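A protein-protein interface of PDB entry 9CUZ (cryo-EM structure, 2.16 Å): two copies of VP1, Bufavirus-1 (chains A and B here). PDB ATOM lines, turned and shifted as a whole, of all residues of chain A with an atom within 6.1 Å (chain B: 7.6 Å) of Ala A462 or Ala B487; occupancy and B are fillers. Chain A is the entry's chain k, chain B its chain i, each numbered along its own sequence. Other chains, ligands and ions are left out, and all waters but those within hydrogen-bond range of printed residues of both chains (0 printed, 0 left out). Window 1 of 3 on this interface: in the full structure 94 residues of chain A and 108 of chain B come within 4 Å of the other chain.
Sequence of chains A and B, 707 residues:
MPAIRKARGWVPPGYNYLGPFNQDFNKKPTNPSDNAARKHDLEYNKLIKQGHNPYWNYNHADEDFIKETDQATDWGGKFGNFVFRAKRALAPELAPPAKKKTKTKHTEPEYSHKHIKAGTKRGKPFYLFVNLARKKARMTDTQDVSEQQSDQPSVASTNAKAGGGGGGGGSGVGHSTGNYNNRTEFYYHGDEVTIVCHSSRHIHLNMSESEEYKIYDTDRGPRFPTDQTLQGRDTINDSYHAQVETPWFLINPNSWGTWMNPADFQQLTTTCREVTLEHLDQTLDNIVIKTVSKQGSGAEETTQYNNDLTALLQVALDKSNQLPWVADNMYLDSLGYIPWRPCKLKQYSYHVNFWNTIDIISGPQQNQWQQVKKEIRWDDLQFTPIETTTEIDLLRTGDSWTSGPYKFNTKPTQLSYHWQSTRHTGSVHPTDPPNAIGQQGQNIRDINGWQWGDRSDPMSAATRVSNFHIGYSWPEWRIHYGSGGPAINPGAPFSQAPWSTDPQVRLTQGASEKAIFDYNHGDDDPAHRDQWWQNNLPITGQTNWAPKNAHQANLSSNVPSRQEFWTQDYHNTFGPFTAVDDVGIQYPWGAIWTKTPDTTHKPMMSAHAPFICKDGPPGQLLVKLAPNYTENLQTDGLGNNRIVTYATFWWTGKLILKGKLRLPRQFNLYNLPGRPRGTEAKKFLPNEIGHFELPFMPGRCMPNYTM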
ATOM      1  N   THR A 422      -8.786  -5.477  19.159  1.00  0.00           N
ATOM      2  CA  THR A 422      -7.684  -6.424  19.238  1.00  0.00           C
ATOM      3  C   THR A 422      -7.764  -7.476  18.135  1.00  0.00           C
ATOM      4  O   THR A 422      -6.729  -7.930  17.650  1.00  0.00           O
ATOM      5  CB  THR A 422      -7.667  -7.082  20.619  1.00  0.00           C
ATOM      6  OG1 THR A 422      -7.516  -6.068  21.614  1.00  0.00           O
ATOM      7  CG2 THR A 422      -6.505  -8.048  20.742  1.00  0.00           C
ATOM      8  N   ARG A 423      -8.964  -7.845  17.706  1.00  0.00           N
ATOM      9  CA  ARG A 423      -9.130  -8.762  16.586  1.00  0.00           C
ATOM     10  C   ARG A 423      -8.843  -8.132  15.227  1.00  0.00           C
ATOM     11  O   ARG A 423      -8.728  -8.866  14.244  1.00  0.00           O
ATOM     12  CB  ARG A 423     -10.543  -9.348  16.607  1.00  0.00           C
ATOM     13  CG  ARG A 423     -10.817 -10.300  17.760  1.00  0.00           C
ATOM     14  CD  ARG A 423     -10.041 -11.591  17.576  1.00  0.00           C
ATOM     15  NE  ARG A 423     -10.474 -12.260  16.357  1.00  0.00           N
ATOM     16  CZ  ARG A 423     -11.539 -13.048  16.273  1.00  0.00           C
ATOM     17  NH1 ARG A 423     -12.268 -13.299  17.347  1.00  0.00           N
ATOM     18  NH2 ARG A 423     -11.869 -13.596  15.117  1.00  0.00           N
ATOM     19  N   GLN A 451      -0.112 -18.800  21.312  1.00  0.00           N
ATOM     20  CA  GLN A 451      -1.513 -18.793  21.810  1.00  0.00           C
ATOM     21  C   GLN A 451      -1.501 -18.618  23.332  1.00  0.00           C
ATOM     22  O   GLN A 451      -0.494 -19.002  23.960  1.00  0.00           O
ATOM     23  CB  GLN A 451      -2.211 -20.092  21.409  1.00  0.00           C
ATOM     24  CG  GLN A 451      -2.354 -20.260  19.903  1.00  0.00           C
ATOM     25  CD  GLN A 451      -3.688 -19.763  19.403  1.00  0.00           C
ATOM     26  OE1 GLN A 451      -4.735 -20.080  19.960  1.00  0.00           O
ATOM     27  NE2 GLN A 451      -3.662 -18.988  18.331  1.00  0.00           N
ATOM     28  N   TRP A 452      -2.574 -18.061  23.897  1.00  0.00           N
ATOM     29  CA  TRP A 452      -2.676 -17.855  25.366  1.00  0.00           C
ATOM     30  C   TRP A 452      -2.834 -19.196  26.089  1.00  0.00           C
ATOM     31  O   TRP A 452      -3.373 -20.139  25.480  1.00  0.00           O
ATOM     32  CB  TRP A 452      -3.841 -16.908  25.693  1.00  0.00           C
ATOM     33  CG  TRP A 452      -3.606 -15.484  25.297  1.00  0.00           C
ATOM     34  CD1 TRP A 452      -4.271 -14.773  24.341  1.00  0.00           C
ATOM     35  CD2 TRP A 452      -2.630 -14.586  25.856  1.00  0.00           C
ATOM     36  NE1 TRP A 452      -3.780 -13.498  24.268  1.00  0.00           N
ATOM     37  CE2 TRP A 452      -2.772 -13.355  25.185  1.00  0.00           C
ATOM     38  CE3 TRP A 452      -1.657 -14.704  26.853  1.00  0.00           C
ATOM     39  CZ2 TRP A 452      -1.973 -12.252  25.481  1.00  0.00           C
ATOM     40  CZ3 TRP A 452      -0.866 -13.615  27.144  1.00  0.00           C
ATOM     41  CH2 TRP A 452      -1.026 -12.407  26.467  1.00  0.00           C
ATOM     42  N   SER A 460      -6.488 -20.347  17.006  1.00  0.00           N
ATOM     43  CA  SER A 460      -7.586 -19.472  16.629  1.00  0.00           C
ATOM     44  C   SER A 460      -7.248 -18.023  16.928  1.00  0.00           C
ATOM     45  O   SER A 460      -6.493 -17.717  17.852  1.00  0.00           O
ATOM     46  CB  SER A 460      -8.883 -19.872  17.335  1.00  0.00           C
ATOM     47  OG  SER A 460      -8.813 -19.676  18.727  1.00  0.00           O
ATOM     48  N   ALA A 461      -7.810 -17.126  16.118  1.00  0.00           N
ATOM     49  CA  ALA A 461      -7.495 -15.711  16.253  1.00  0.00           C
ATOM     50  C   ALA A 461      -7.882 -15.185  17.628  1.00  0.00           C
ATOM     51  O   ALA A 461      -7.197 -14.320  18.180  1.00  0.00           O
ATOM     52  CB  ALA A 461      -8.191 -14.913  15.153  1.00  0.00           C
ATOM     53  N   ALA A 462      -8.967 -15.702  18.200  1.00  0.00           N
ATOM     54  CA  ALA A 462      -9.436 -15.205  19.488  1.00  0.00           C
ATOM     55  C   ALA A 462      -8.427 -15.459  20.600  1.00  0.00           C
ATOM     56  O   ALA A 462      -8.267 -14.627  21.493  1.00  0.00           O
ATOM     57  CB  ALA A 462     -10.775 -15.843  19.833  1.00  0.00           C
ATOM     58  N   THR A 463      -7.755 -16.602  20.577  1.00  0.00           N
ATOM     59  CA  THR A 463      -6.761 -16.942  21.582  1.00  0.00           C
ATOM     60  C   THR A 463      -5.333 -16.616  21.154  1.00  0.00           C
ATOM     61  O   THR A 463      -4.393 -16.994  21.852  1.00  0.00           O
ATOM     62  CB  THR A 463      -6.899 -18.408  21.986  1.00  0.00           C
ATOM     63  OG1 THR A 463      -6.809 -19.244  20.828  1.00  0.00           O
ATOM     64  CG2 THR A 463      -8.228 -18.641  22.694  1.00  0.00           C
ATOM     65  N   ARG A 464      -5.147 -15.967  20.009  1.00  0.00           N
ATOM     66  CA  ARG A 464      -3.823 -15.475  19.666  1.00  0.00           C
ATOM     67  C   ARG A 464      -3.338 -14.483  20.716  1.00  0.00           C
ATOM     68  O   ARG A 464      -4.083 -13.607  21.157  1.00  0.00           O
ATOM     69  CB  ARG A 464      -3.815 -14.795  18.300  1.00  0.00           C
ATOM     70  CG  ARG A 464      -2.437 -14.297  17.958  1.00  0.00           C
ATOM     71  CD  ARG A 464      -2.324 -13.576  16.655  1.00  0.00           C
ATOM     72  NE  ARG A 464      -3.074 -12.332  16.626  1.00  0.00           N
ATOM     73  CZ  ARG A 464      -2.665 -11.191  17.165  1.00  0.00           C
ATOM     74  NH1 ARG A 464      -3.402 -10.105  17.073  1.00  0.00           N
ATOM     75  NH2 ARG A 464      -1.534 -11.140  17.825  1.00  0.00           N
ATOM     76  N   HIS A 469      -4.129  -4.500  24.653  1.00  0.00           N
ATOM     77  CA  HIS A 469      -5.552  -4.740  24.494  1.00  0.00           C
ATOM     78  C   HIS A 469      -6.269  -3.411  24.316  1.00  0.00           C
ATOM     79  O   HIS A 469      -6.029  -2.464  25.067  1.00  0.00           O
ATOM     80  CB  HIS A 469      -6.122  -5.524  25.675  1.00  0.00           C
ATOM     81  CG  HIS A 469      -7.465  -6.111  25.393  1.00  0.00           C
ATOM     82  ND1 HIS A 469      -8.637  -5.406  25.538  1.00  0.00           N
ATOM     83  CD2 HIS A 469      -7.812  -7.319  24.894  1.00  0.00           C
ATOM     84  CE1 HIS A 469      -9.651  -6.169  25.181  1.00  0.00           C
ATOM     85  NE2 HIS A 469      -9.177  -7.336  24.783  1.00  0.00           N
ATOM     86  N   THR B 235     -17.505 -20.750  21.528  1.00  0.00           N
ATOM     87  CA  THR B 235     -17.369 -19.613  20.629  1.00  0.00           C
ATOM     88  C   THR B 235     -16.020 -18.918  20.765  1.00  0.00           C
ATOM     89  O   THR B 235     -15.704 -18.067  19.930  1.00  0.00           O
ATOM     90  CB  THR B 235     -18.492 -18.596  20.851  1.00  0.00           C
ATOM     91  OG1 THR B 235     -18.471 -18.135  22.204  1.00  0.00           O
ATOM     92  CG2 THR B 235     -19.838 -19.213  20.550  1.00  0.00           C
ATOM     93  N   ILE B 236     -15.220 -19.262  21.779  1.00  0.00           N
ATOM     94  CA  ILE B 236     -13.849 -18.773  21.887  1.00  0.00           C
ATOM     95  C   ILE B 236     -12.964 -19.294  20.763  1.00  0.00           C
ATOM     96  O   ILE B 236     -11.830 -18.838  20.604  1.00  0.00           O
ATOM     97  CB  ILE B 236     -13.254 -19.158  23.259  1.00  0.00           C
ATOM     98  CG1 ILE B 236     -11.912 -18.465  23.502  1.00  0.00           C
ATOM     99  CG2 ILE B 236     -13.064 -20.658  23.352  1.00  0.00           C
ATOM    100  CD1 ILE B 236     -11.391 -18.597  24.920  1.00  0.00           C
ATOM    101  N   ASN B 237     -13.465 -20.219  19.960  1.00  0.00           N
ATOM    102  CA  ASN B 237     -12.723 -20.849  18.872  1.00  0.00           C
ATOM    103  C   ASN B 237     -12.831 -20.058  17.574  1.00  0.00           C
ATOM    104  O   ASN B 237     -12.437 -20.538  16.513  1.00  0.00           O
ATOM    105  CB  ASN B 237     -13.206 -22.283  18.695  1.00  0.00           C
ATOM    106  CG  ASN B 237     -12.809 -23.171  19.860  1.00  0.00           C
ATOM    107  OD1 ASN B 237     -11.839 -22.896  20.553  1.00  0.00           O
ATOM    108  ND2 ASN B 237     -13.572 -24.221  20.093  1.00  0.00           N
ATOM    109  N   ASP B 238     -13.410 -18.865  17.624  1.00  0.00           N
ATOM    110  CA  ASP B 238     -13.685 -18.050  16.448  1.00  0.00           C
ATOM    111  C   ASP B 238     -12.411 -17.502  15.816  1.00  0.00           C
ATOM    112  O   ASP B 238     -11.640 -16.795  16.470  1.00  0.00           O
ATOM    113  CB  ASP B 238     -14.585 -16.886  16.841  1.00  0.00           C
ATOM    114  CG  ASP B 238     -14.855 -15.963  15.696  1.00  0.00           C
ATOM    115  OD1 ASP B 238     -15.523 -16.386  14.742  1.00  0.00           O
ATOM    116  OD2 ASP B 238     -14.386 -14.818  15.745  1.00  0.00           O
ATOM    117  N   SER B 239     -12.181 -17.850  14.553  1.00  0.00           N
ATOM    118  CA  SER B 239     -11.183 -17.200  13.708  1.00  0.00           C
ATOM    119  C   SER B 239     -11.750 -16.218  12.679  1.00  0.00           C
ATOM    120  O   SER B 239     -10.991 -15.748  11.836  1.00  0.00           O
ATOM    121  CB  SER B 239     -10.296 -18.237  13.026  1.00  0.00           C
ATOM    122  OG  SER B 239      -9.509 -18.896  13.990  1.00  0.00           O
ATOM    123  N   TYR B 240     -13.057 -15.960  12.659  1.00  0.00           N
ATOM    124  CA  TYR B 240     -13.623 -15.126  11.600  1.00  0.00           C
ATOM    125  C   TYR B 240     -12.911 -13.782  11.506  1.00  0.00           C
ATOM    126  O   TYR B 240     -12.559 -13.175  12.519  1.00  0.00           O
ATOM    127  CB  TYR B 240     -15.114 -14.874  11.827  1.00  0.00           C
ATOM    128  CG  TYR B 240     -15.716 -13.935  10.802  1.00  0.00           C
ATOM    129  CD1 TYR B 240     -16.118 -14.397   9.560  1.00  0.00           C
ATOM    130  CD2 TYR B 240     -15.811 -12.571  11.051  1.00  0.00           C
ATOM    131  CE1 TYR B 240     -16.644 -13.545   8.620  1.00  0.00           C
ATOM    132  CE2 TYR B 240     -16.326 -11.710  10.110  1.00  0.00           C
ATOM    133  CZ  TYR B 240     -16.745 -12.203   8.899  1.00  0.00           C
ATOM    134  OH  TYR B 240     -17.265 -11.349   7.961  1.00  0.00           O
ATOM    135  N   TYR B 331       2.031 -15.322  14.656  1.00  0.00           N
ATOM    136  CA  TYR B 331       1.918 -16.605  13.967  1.00  0.00           C
ATOM    137  C   TYR B 331       3.274 -17.220  13.626  1.00  0.00           C
ATOM    138  O   TYR B 331       3.323 -18.196  12.878  1.00  0.00           O
ATOM    139  CB  TYR B 331       1.008 -16.525  12.741  1.00  0.00           C
ATOM    140  CG  TYR B 331      -0.412 -16.234  13.155  1.00  0.00           C
ATOM    141  CD1 TYR B 331      -1.206 -17.228  13.702  1.00  0.00           C
ATOM    142  CD2 TYR B 331      -0.973 -14.986  12.957  1.00  0.00           C
ATOM    143  CE1 TYR B 331      -2.496 -16.970  14.095  1.00  0.00           C
ATOM    144  CE2 TYR B 331      -2.263 -14.720  13.329  1.00  0.00           C
ATOM    145  CZ  TYR B 331      -3.021 -15.712  13.901  1.00  0.00           C
ATOM    146  OH  TYR B 331      -4.310 -15.448  14.267  1.00  0.00           O
ATOM    147  N   TRP B 477      -8.121 -15.253  32.270  1.00  0.00           N
ATOM    148  CA  TRP B 477      -8.656 -15.620  30.970  1.00  0.00           C
ATOM    149  C   TRP B 477     -10.005 -14.943  30.757  1.00  0.00           C
ATOM    150  O   TRP B 477     -11.042 -15.577  30.579  1.00  0.00           O
ATOM    151  CB  TRP B 477      -8.703 -17.127  30.738  1.00  0.00           C
ATOM    152  CG  TRP B 477      -7.334 -17.773  30.898  1.00  0.00           C
ATOM    153  CD1 TRP B 477      -6.986 -18.713  31.813  1.00  0.00           C
ATOM    154  CD2 TRP B 477      -6.101 -17.330  30.311  1.00  0.00           C
ATOM    155  NE1 TRP B 477      -5.650 -19.001  31.724  1.00  0.00           N
ATOM    156  CE2 TRP B 477      -5.078 -18.148  30.822  1.00  0.00           C
ATOM    157  CE3 TRP B 477      -5.770 -16.359  29.364  1.00  0.00           C
ATOM    158  CZ2 TRP B 477      -3.756 -18.029  30.416  1.00  0.00           C
ATOM    159  CZ3 TRP B 477      -4.463 -16.245  28.969  1.00  0.00           C
ATOM    160  CH2 TRP B 477      -3.469 -17.074  29.494  1.00  0.00           C
ATOM    161  N   ARG B 478      -9.965 -13.628  30.880  1.00  0.00           N
ATOM    162  CA  ARG B 478     -10.981 -12.704  30.405  1.00  0.00           C
ATOM    163  C   ARG B 478     -11.216 -12.875  28.909  1.00  0.00           C
ATOM    164  O   ARG B 478     -10.269 -12.825  28.122  1.00  0.00           O
ATOM    165  CB  ARG B 478     -10.485 -11.296  30.713  1.00  0.00           C
ATOM    166  CG  ARG B 478     -11.364 -10.171  30.305  1.00  0.00           C
ATOM    167  CD  ARG B 478     -12.612 -10.315  31.015  1.00  0.00           C
ATOM    168  NE  ARG B 478     -13.463  -9.149  30.895  1.00  0.00           N
ATOM    169  CZ  ARG B 478     -14.717  -9.143  31.290  1.00  0.00           C
ATOM    170  NH1 ARG B 478     -15.433  -8.045  31.202  1.00  0.00           N
ATOM    171  NH2 ARG B 478     -15.239 -10.243  31.793  1.00  0.00           N
ATOM    172  N   ILE B 479     -12.469 -13.050  28.511  1.00  0.00           N
ATOM    173  CA  ILE B 479     -12.826 -13.075  27.097  1.00  0.00           C
ATOM    174  C   ILE B 479     -13.618 -11.813  26.785  1.00  0.00           C
ATOM    175  O   ILE B 479     -14.691 -11.588  27.346  1.00  0.00           O
ATOM    176  CB  ILE B 479     -13.636 -14.322  26.740  1.00  0.00           C
ATOM    177  CG1 ILE B 479     -12.845 -15.585  27.027  1.00  0.00           C
ATOM    178  CG2 ILE B 479     -13.927 -14.318  25.263  1.00  0.00           C
ATOM    179  CD1 ILE B 479     -13.694 -16.804  26.962  1.00  0.00           C
ATOM    180  N   HIS B 480     -13.081 -10.990  25.891  1.00  0.00           N
ATOM    181  CA  HIS B 480     -13.633  -9.664  25.643  1.00  0.00           C
ATOM    182  C   HIS B 480     -14.869  -9.651  24.737  1.00  0.00           C
ATOM    183  O   HIS B 480     -15.850  -8.990  25.069  1.00  0.00           O
ATOM    184  CB  HIS B 480     -12.510  -8.743  25.162  1.00  0.00           C
ATOM    185  CG  HIS B 480     -12.973  -7.473  24.523  1.00  0.00           C
ATOM    186  ND1 HIS B 480     -14.002  -6.708  25.021  1.00  0.00           N
ATOM    187  CD2 HIS B 480     -12.438  -6.763  23.503  1.00  0.00           C
ATOM    188  CE1 HIS B 480     -14.160  -5.645  24.257  1.00  0.00           C
ATOM    189  NE2 HIS B 480     -13.202  -5.635  23.354  1.00  0.00           N
ATOM    190  N   TYR B 481     -14.883 -10.369  23.620  1.00  0.00           N
ATOM    191  CA  TYR B 481     -16.013 -10.228  22.685  1.00  0.00           C
ATOM    192  C   TYR B 481     -16.219  -8.785  22.246  1.00  0.00           C
ATOM    193  O   TYR B 481     -17.239  -8.172  22.566  1.00  0.00           O
ATOM    194  CB  TYR B 481     -17.342 -10.755  23.255  1.00  0.00           C
ATOM    195  CG  TYR B 481     -17.425 -12.254  23.399  1.00  0.00           C
ATOM    196  CD1 TYR B 481     -17.796 -13.045  22.325  1.00  0.00           C
ATOM    197  CD2 TYR B 481     -17.143 -12.878  24.603  1.00  0.00           C
ATOM    198  CE1 TYR B 481     -17.863 -14.411  22.437  1.00  0.00           C
ATOM    199  CE2 TYR B 481     -17.215 -14.248  24.726  1.00  0.00           C
ATOM    200  CZ  TYR B 481     -17.572 -15.007  23.636  1.00  0.00           C
ATOM    201  OH  TYR B 481     -17.647 -16.367  23.744  1.00  0.00           O
ATOM    202  N   GLY B 482     -15.255  -8.230  21.518  1.00  0.00           N
ATOM    203  CA  GLY B 482     -15.364  -6.897  20.983  1.00  0.00           C
ATOM    204  C   GLY B 482     -16.027  -6.909  19.620  1.00  0.00           C
ATOM    205  O   GLY B 482     -16.599  -7.897  19.173  1.00  0.00           O
ATOM    206  N   GLY B 484     -15.491  -7.426  16.013  1.00  0.00           N
ATOM    207  CA  GLY B 484     -14.487  -8.289  15.434  1.00  0.00           C
ATOM    208  C   GLY B 484     -14.305  -9.599  16.163  1.00  0.00           C
ATOM    209  O   GLY B 484     -13.497 -10.424  15.726  1.00  0.00           O
ATOM    210  N   GLY B 485     -15.061  -9.830  17.231  1.00  0.00           N
ATOM    211  CA  GLY B 485     -15.115 -11.122  17.869  1.00  0.00           C
ATOM    212  C   GLY B 485     -14.413 -11.212  19.207  1.00  0.00           C
ATOM    213  O   GLY B 485     -13.813 -10.254  19.693  1.00  0.00           O
ATOM    214  N   PRO B 486     -14.504 -12.379  19.838  1.00  0.00           N
ATOM    215  CA  PRO B 486     -13.868 -12.562  21.146  1.00  0.00           C
ATOM    216  C   PRO B 486     -12.353 -12.514  21.058  1.00  0.00           C
ATOM    217  O   PRO B 486     -11.749 -12.897  20.058  1.00  0.00           O
ATOM    218  CB  PRO B 486     -14.361 -13.942  21.585  1.00  0.00           C
ATOM    219  CG  PRO B 486     -14.670 -14.637  20.312  1.00  0.00           C
ATOM    220  CD  PRO B 486     -15.213 -13.590  19.404  1.00  0.00           C
ATOM    221  N   ALA B 487     -11.749 -12.032  22.144  1.00  0.00           N
ATOM    222  CA  ALA B 487     -10.276 -11.981  22.236  1.00  0.00           C
ATOM    223  C   ALA B 487      -9.907 -12.071  23.717  1.00  0.00           C
ATOM    224  O   ALA B 487     -10.650 -11.511  24.540  1.00  0.00           O
ATOM    225  CB  ALA B 487      -9.762 -10.707  21.620  1.00  0.00           C
ATOM    226  N   ILE B 488      -8.808 -12.753  24.035  1.00  0.00           N
ATOM    227  CA  ILE B 488      -8.348 -12.857  25.447  1.00  0.00           C
ATOM    228  C   ILE B 488      -7.860 -11.488  25.926  1.00  0.00           C
ATOM    229  O   ILE B 488      -7.018 -10.895  25.235  1.00  0.00           O
ATOM    230  CB  ILE B 488      -7.230 -13.912  25.565  1.00  0.00           C
ATOM    231  CG1 ILE B 488      -7.758 -15.328  25.322  1.00  0.00           C
ATOM    232  CG2 ILE B 488      -6.516 -13.795  26.905  1.00  0.00           C
ATOM    233  CD1 ILE B 488      -8.918 -15.710  26.210  1.00  0.00           C
ATOM    234  N   ASN B 489      -8.404 -10.982  27.038  1.00  0.00           N
ATOM    235  CA  ASN B 489      -7.847  -9.732  27.625  1.00  0.00           C
ATOM    236  C   ASN B 489      -6.841 -10.212  28.675  1.00  0.00           C
ATOM    237  O   ASN B 489      -7.273 -10.657  29.750  1.00  0.00           O
ATOM    238  CB  ASN B 489      -8.936  -8.776  28.119  1.00  0.00           C
ATOM    239  CG  ASN B 489      -8.404  -7.401  28.462  1.00  0.00           C
ATOM    240  OD1 ASN B 489      -7.194  -7.195  28.523  1.00  0.00           O
ATOM    241  ND2 ASN B 489      -9.298  -6.454  28.686  1.00  0.00           N
ATOM    242  N   PRO B 490      -5.520 -10.136  28.410  1.00  0.00           N
ATOM    243  CA  PRO B 490      -4.524 -10.744  29.305  1.00  0.00           C
ATOM    244  C   PRO B 490      -4.333 -10.121  30.692  1.00  0.00           C
ATOM    245  O   PRO B 490      -4.289  -8.910  30.784  1.00  0.00           O
ATOM    246  CB  PRO B 490      -3.196 -10.561  28.548  1.00  0.00           C
ATOM    247  CG  PRO B 490      -3.575 -10.105  27.152  1.00  0.00           C
ATOM    248  CD  PRO B 490      -4.923  -9.435  27.279  1.00  0.00           C
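Of chain B, only Ile B236 (3.3 Å), Asp B238 (3.4 Å), Pro B486 (3.1 Å), Ala B487 (3.4 Å) and Ile B488 (3.2 Å) come within 4 Å of Ala A462.
Of chain A, only Ala A462 comes within 4 Å of Ala B487.
Ala A461 touches just these residues of chain B: Asp B238, Ser B239 and Tyr B331.
Printed residues of chain B within 4 Å of Arg A464: Tyr B331 (3.5 Å).
Of the printed residues of chain B, Trp A452 touches Trp B477 (3.4 Å), Ile B488 (3.3 Å) and Pro B490 (3.2 Å).
Of the printed residues of chain B, Thr A463 touches Ile B236 (3.8 Å).
Printed residues of chain A within 4 Å of Ile B236: Ser A460 (3.7 Å), Ala A462 (3.3 Å) and Thr A463 (3.8 Å).
Printed residues of chain A within 4 Å of Asn B489: His A469 (3.3 Å).
The nearest residue of chain B that does not touch Ala A462 is Asn B237 (5.1 Å).
The nearest residue of chain A that does not touch Ala B487 is Arg A423 (4.02 Å).
The nearest printed residue of chain B that does not touch Arg A464 is Ile B488 (5.4 Å).
The backbone NH of Tyr B240 lies within hydrogen-bond range of the side-chain carboxylate of Asp B238 (3.3 Å).
The backbone carbonyl oxygen (O) of Arg A464 sits at hydrogen-bond distance from the indole nitrogen (NE1) of Trp A452 (3.1 Å).
The side-chain amide nitrogen (NE2) of Gln A451 is in hydrogen-bond range of the backbone carbonyl oxygen (O) of Ser A460, at 3.1 Å.
N of His B480 is in hydrogen-bond range of O of Ala B487 (2.8 Å).
The side-chain hydroxyl (OG) of Ser A460 is in hydrogen-bond range of the side-chain hydroxyl (OG1) of Thr A463 (2.9 Å).
The backbone NH (N) of Asn B489 sits at hydrogen-bond distance from the backbone carbonyl oxygen (O) of Arg B478, 2.8 Å away.
No position is printed for both chains.
Among the printed residues, merely in contact across the chains: Ala A462 with Pro B486, Trp A452 with Pro B490, Arg A423 with Gly B484, Ala A462 with Ile B236, His A469 with His B480, Ser A460 with Ser B239, Trp A452 with Ile B488, Trp A452 with Trp B477, Ala A462 with Ala B487, Arg A464 with Tyr B331, Arg A423 with Gly B485, Arg A423 with Ser B239, Ser A460 with Ile B236, His A469 with Ile B488, Ser A460 with Asn B237, Ala A461 with Tyr B331, Thr A463 with Ile B236 and Ala A461 with Asp B238.
The side-chain amide nitrogen (ND2) of Asn B489 sits at hydrogen-bond distance from a ring nitrogen (ND1) of His A469.
N of Ala A461 lies within hydrogen-bond range of OG of Ser B239 (3.2 Å).
O of Pro B486 is in hydrogen-bond range of NH1 of Arg A423.
The guanidinium group (NH2) of Arg A423 is in salt-bridge range of the side-chain carboxylate (OD2) of Asp B238 (2.9 Å).
O of Ala A462 is in hydrogen-bond range of N of Ile B488, 3.2 Å away.
The backbone carbonyl oxygen of Tyr B240 is in hydrogen-bond range of the guanidinium group of Arg A423.
The backbone carbonyl oxygen (O) of Asp B238 sits at hydrogen-bond distance from the backbone NH (N) of Ala A462 (3.4 Å).
Hydrophobic or aromatic side chains of chain B within 4 Å of the printed part of chain A: Ile B236, Tyr B331, Trp B477, His B480, Pro B486, Ile B488 and Pro B490.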
